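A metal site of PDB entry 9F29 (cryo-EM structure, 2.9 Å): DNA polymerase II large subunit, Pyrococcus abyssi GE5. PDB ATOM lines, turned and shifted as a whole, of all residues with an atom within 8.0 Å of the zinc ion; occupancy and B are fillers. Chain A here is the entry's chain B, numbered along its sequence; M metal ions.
The nearest printed residue that does not touch the zinc ion is Val 755 (4.7 Å).
The zinc ion is bound by the side-chain sulfur (SG) of Cys 734, the side-chain sulfur (SG) of Cys 731, the side-chain sulfur (SG) of Cys 753 and the side-chain sulfur (SG) of Cys 750. The zinc ion has four donor atoms within binding distance.
SG of Cys 731 sits close to N of Arg 733 (3.8 Å). The backbone NH (N) of Cys 731 is in hydrogen-bond range of the backbone carbonyl oxygen (O) of Ala 736 (3.4 Å). The side-chain sulfur of Cys 753 sits close to the guanidinium group of Arg 733 (3.5 Å). The backbone NH (N) of Cys 750 lies within hydrogen-bond range of the backbone carbonyl oxygen (O) of Val 755, 3.2 Å away.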
ATOM      1  N   VAL A 730       1.520 -27.683  11.562  1.00  0.00           N
ATOM      2  CA  VAL A 730       0.726 -27.229  10.428  1.00  0.00           C
ATOM      3  C   VAL A 730      -0.652 -27.878  10.481  1.00  0.00           C
ATOM      4  O   VAL A 730      -0.830 -28.961  11.059  1.00  0.00           O
ATOM      5  CB  VAL A 730       1.421 -27.543   9.091  1.00  0.00           C
ATOM      6  CG1 VAL A 730       2.834 -26.990   9.087  1.00  0.00           C
ATOM      7  CG2 VAL A 730       1.439 -29.037   8.832  1.00  0.00           C
ATOM      8  N   CYS A 731      -1.621 -27.198   9.878  1.00  0.00           N
ATOM      9  CA  CYS A 731      -2.960 -27.754   9.687  1.00  0.00           C
ATOM     10  C   CYS A 731      -3.127 -28.110   8.221  1.00  0.00           C
ATOM     11  O   CYS A 731      -2.964 -27.231   7.365  1.00  0.00           O
ATOM     12  CB  CYS A 731      -4.022 -26.762  10.115  1.00  0.00           C
ATOM     13  SG  CYS A 731      -5.712 -27.303   9.791  1.00  0.00           S
ATOM     14  N   PRO A 732      -3.443 -29.367   7.888  1.00  0.00           N
ATOM     15  CA  PRO A 732      -3.445 -29.762   6.469  1.00  0.00           C
ATOM     16  C   PRO A 732      -4.475 -29.045   5.612  1.00  0.00           C
ATOM     17  O   PRO A 732      -4.326 -29.025   4.386  1.00  0.00           O
ATOM     18  CB  PRO A 732      -3.737 -31.267   6.535  1.00  0.00           C
ATOM     19  CG  PRO A 732      -4.341 -31.492   7.877  1.00  0.00           C
ATOM     20  CD  PRO A 732      -3.734 -30.480   8.786  1.00  0.00           C
ATOM     21  N   ARG A 733      -5.517 -28.445   6.201  1.00  0.00           N
ATOM     22  CA  ARG A 733      -6.562 -27.792   5.422  1.00  0.00           C
ATOM     23  C   ARG A 733      -6.335 -26.299   5.243  1.00  0.00           C
ATOM     24  O   ARG A 733      -6.236 -25.822   4.102  1.00  0.00           O
ATOM     25  CB  ARG A 733      -7.929 -28.036   6.075  1.00  0.00           C
ATOM     26  CG  ARG A 733      -8.226 -29.499   6.328  1.00  0.00           C
ATOM     27  CD  ARG A 733      -9.607 -29.702   6.938  1.00  0.00           C
ATOM     28  NE  ARG A 733     -10.664 -29.297   6.018  1.00  0.00           N
ATOM     29  CZ  ARG A 733     -11.557 -28.350   6.275  1.00  0.00           C
ATOM     30  NH1 ARG A 733     -11.546 -27.673   7.401  1.00  0.00           N
ATOM     31  NH2 ARG A 733     -12.485 -28.073   5.361  1.00  0.00           N
ATOM     32  N   CYS A 734      -6.244 -25.536   6.337  1.00  0.00           N
ATOM     33  CA  CYS A 734      -6.092 -24.090   6.226  1.00  0.00           C
ATOM     34  C   CYS A 734      -4.639 -23.626   6.211  1.00  0.00           C
ATOM     35  O   CYS A 734      -4.391 -22.443   5.980  1.00  0.00           O
ATOM     36  CB  CYS A 734      -6.839 -23.387   7.375  1.00  0.00           C
ATOM     37  SG  CYS A 734      -6.244 -23.760   9.030  1.00  0.00           S
ATOM     38  N   ASN A 735      -3.681 -24.528   6.456  1.00  0.00           N
ATOM     39  CA  ASN A 735      -2.247 -24.224   6.392  1.00  0.00           C
ATOM     40  C   ASN A 735      -1.884 -23.074   7.348  1.00  0.00           C
ATOM     41  O   ASN A 735      -1.444 -22.002   6.930  1.00  0.00           O
ATOM     42  CB  ASN A 735      -1.815 -23.906   4.960  1.00  0.00           C
ATOM     43  CG  ASN A 735      -2.213 -24.986   3.989  1.00  0.00           C
ATOM     44  OD1 ASN A 735      -3.391 -25.308   3.837  1.00  0.00           O
ATOM     45  ND2 ASN A 735      -1.220 -25.579   3.321  1.00  0.00           N
ATOM     46  N   ALA A 736      -2.069 -23.337   8.639  1.00  0.00           N
ATOM     47  CA  ALA A 736      -1.759 -22.374   9.680  1.00  0.00           C
ATOM     48  C   ALA A 736      -0.644 -22.917  10.559  1.00  0.00           C
ATOM     49  O   ALA A 736      -0.649 -24.098  10.916  1.00  0.00           O
ATOM     50  CB  ALA A 736      -2.992 -22.061  10.534  1.00  0.00           C
ATOM     51  N   TYR A 738       1.521 -23.079  14.012  1.00  0.00           N
ATOM     52  CA  TYR A 738       1.382 -22.898  15.450  1.00  0.00           C
ATOM     53  C   TYR A 738       2.636 -23.419  16.150  1.00  0.00           C
ATOM     54  O   TYR A 738       3.042 -24.572  15.910  1.00  0.00           O
ATOM     55  CB  TYR A 738       0.141 -23.614  15.984  1.00  0.00           C
ATOM     56  CG  TYR A 738      -1.170 -23.024  15.515  1.00  0.00           C
ATOM     57  CD1 TYR A 738      -1.622 -21.803  16.015  1.00  0.00           C
ATOM     58  CD2 TYR A 738      -1.952 -23.686  14.589  1.00  0.00           C
ATOM     59  CE1 TYR A 738      -2.809 -21.266  15.581  1.00  0.00           C
ATOM     60  CE2 TYR A 738      -3.153 -23.151  14.154  1.00  0.00           C
ATOM     61  CZ  TYR A 738      -3.568 -21.938  14.660  1.00  0.00           C
ATOM     62  OH  TYR A 738      -4.763 -21.405  14.232  1.00  0.00           O
ATOM     63  N   THR A 749      -5.032 -29.506  18.099  1.00  0.00           N
ATOM     64  CA  THR A 749      -6.193 -29.543  17.213  1.00  0.00           C
ATOM     65  C   THR A 749      -6.490 -28.126  16.751  1.00  0.00           C
ATOM     66  O   THR A 749      -6.406 -27.183  17.547  1.00  0.00           O
ATOM     67  CB  THR A 749      -7.407 -30.155  17.911  1.00  0.00           C
ATOM     68  OG1 THR A 749      -7.075 -31.462  18.391  1.00  0.00           O
ATOM     69  CG2 THR A 749      -8.580 -30.261  16.957  1.00  0.00           C
ATOM     70  N   CYS A 750      -6.824 -27.977  15.482  1.00  0.00           N
ATOM     71  CA  CYS A 750      -7.053 -26.656  14.897  1.00  0.00           C
ATOM     72  C   CYS A 750      -8.362 -26.090  15.414  1.00  0.00           C
ATOM     73  O   CYS A 750      -9.404 -26.736  15.281  1.00  0.00           O
ATOM     74  CB  CYS A 750      -7.059 -26.732  13.376  1.00  0.00           C
ATOM     75  SG  CYS A 750      -7.186 -25.146  12.517  1.00  0.00           S
ATOM     76  N   PRO A 751      -8.370 -24.891  16.000  1.00  0.00           N
ATOM     77  CA  PRO A 751      -9.635 -24.343  16.526  1.00  0.00           C
ATOM     78  C   PRO A 751     -10.690 -24.115  15.461  1.00  0.00           C
ATOM     79  O   PRO A 751     -11.888 -24.273  15.748  1.00  0.00           O
ATOM     80  CB  PRO A 751      -9.192 -23.016  17.172  1.00  0.00           C
ATOM     81  CG  PRO A 751      -7.914 -22.670  16.510  1.00  0.00           C
ATOM     82  CD  PRO A 751      -7.239 -23.967  16.198  1.00  0.00           C
ATOM     83  N   LYS A 752     -10.295 -23.762  14.244  1.00  0.00           N
ATOM     84  CA  LYS A 752     -11.272 -23.483  13.193  1.00  0.00           C
ATOM     85  C   LYS A 752     -11.683 -24.741  12.441  1.00  0.00           C
ATOM     86  O   LYS A 752     -12.820 -24.845  11.974  1.00  0.00           O
ATOM     87  CB  LYS A 752     -10.706 -22.446  12.227  1.00  0.00           C
ATOM     88  CG  LYS A 752     -10.384 -21.111  12.861  1.00  0.00           C
ATOM     89  CD  LYS A 752      -9.560 -20.235  11.923  1.00  0.00           C
ATOM     90  CE  LYS A 752     -10.386 -19.763  10.741  1.00  0.00           C
ATOM     91  NZ  LYS A 752      -9.607 -18.853   9.857  1.00  0.00           N
ATOM     92  N   CYS A 753     -10.774 -25.707  12.318  1.00  0.00           N
ATOM     93  CA  CYS A 753     -11.021 -26.896  11.508  1.00  0.00           C
ATOM     94  C   CYS A 753     -11.406 -28.114  12.331  1.00  0.00           C
ATOM     95  O   CYS A 753     -12.069 -29.013  11.792  1.00  0.00           O
ATOM     96  CB  CYS A 753      -9.788 -27.230  10.675  1.00  0.00           C
ATOM     97  SG  CYS A 753      -9.319 -25.976   9.463  1.00  0.00           S
ATOM     98  N   ASN A 754     -11.003 -28.176  13.607  1.00  0.00           N
ATOM     99  CA  ASN A 754     -11.202 -29.351  14.455  1.00  0.00           C
ATOM    100  C   ASN A 754     -10.582 -30.604  13.830  1.00  0.00           C
ATOM    101  O   ASN A 754     -11.144 -31.698  13.905  1.00  0.00           O
ATOM    102  CB  ASN A 754     -12.688 -29.579  14.761  1.00  0.00           C
ATOM    103  CG  ASN A 754     -13.173 -28.752  15.933  1.00  0.00           C
ATOM    104  OD1 ASN A 754     -12.382 -28.085  16.600  1.00  0.00           O
ATOM    105  ND2 ASN A 754     -14.472 -28.797  16.183  1.00  0.00           N
ATOM    106  N   VAL A 755      -9.418 -30.436  13.214  1.00  0.00           N
ATOM    107  CA  VAL A 755      -8.701 -31.539  12.590  1.00  0.00           C
ATOM    108  C   VAL A 755      -7.348 -31.701  13.262  1.00  0.00           C
ATOM    109  O   VAL A 755      -6.838 -30.791  13.931  1.00  0.00           O
ATOM    110  CB  VAL A 755      -8.518 -31.334  11.071  1.00  0.00           C
ATOM    111  CG1 VAL A 755      -9.870 -31.117  10.404  1.00  0.00           C
ATOM    112  CG2 VAL A 755      -7.597 -30.170  10.799  1.00  0.00           C
ATOM    113  N   LYS A 756      -6.761 -32.877  13.085  1.00  0.00           N
ATOM    114  CA  LYS A 756      -5.501 -33.218  13.741  1.00  0.00           C
ATOM    115  C   LYS A 756      -4.343 -32.500  13.060  1.00  0.00           C
ATOM    116  O   LYS A 756      -4.230 -32.487  11.837  1.00  0.00           O
ATOM    117  CB  LYS A 756      -5.275 -34.733  13.690  1.00  0.00           C
ATOM    118  CG  LYS A 756      -4.253 -35.231  14.696  1.00  0.00           C
ATOM    119  CD  LYS A 756      -4.731 -35.023  16.120  1.00  0.00           C
ATOM    120  CE  LYS A 756      -5.916 -35.924  16.430  1.00  0.00           C
ATOM    121  NZ  LYS A 756      -5.528 -37.354  16.494  1.00  0.00           N
ATOM    122  N   LEU A 757      -3.478 -31.893  13.875  1.00  0.00           N
ATOM    123  CA  LEU A 757      -2.328 -31.158  13.362  1.00  0.00           C
ATOM    124  C   LEU A 757      -1.167 -32.104  13.081  1.00  0.00           C
ATOM    125  O   LEU A 757      -1.055 -33.195  13.641  1.00  0.00           O
ATOM    126  CB  LEU A 757      -1.896 -30.083  14.356  1.00  0.00           C
ATOM    127  CG  LEU A 757      -2.492 -28.696  14.146  1.00  0.00           C
ATOM    128  CD1 LEU A 757      -3.989 -28.745  14.311  1.00  0.00           C
ATOM    129  CD2 LEU A 757      -1.891 -27.713  15.135  1.00  0.00           C
HETATM  130 ZN    ZN M   1      -7.159 -25.531  10.217  1.00  0.00          ZN
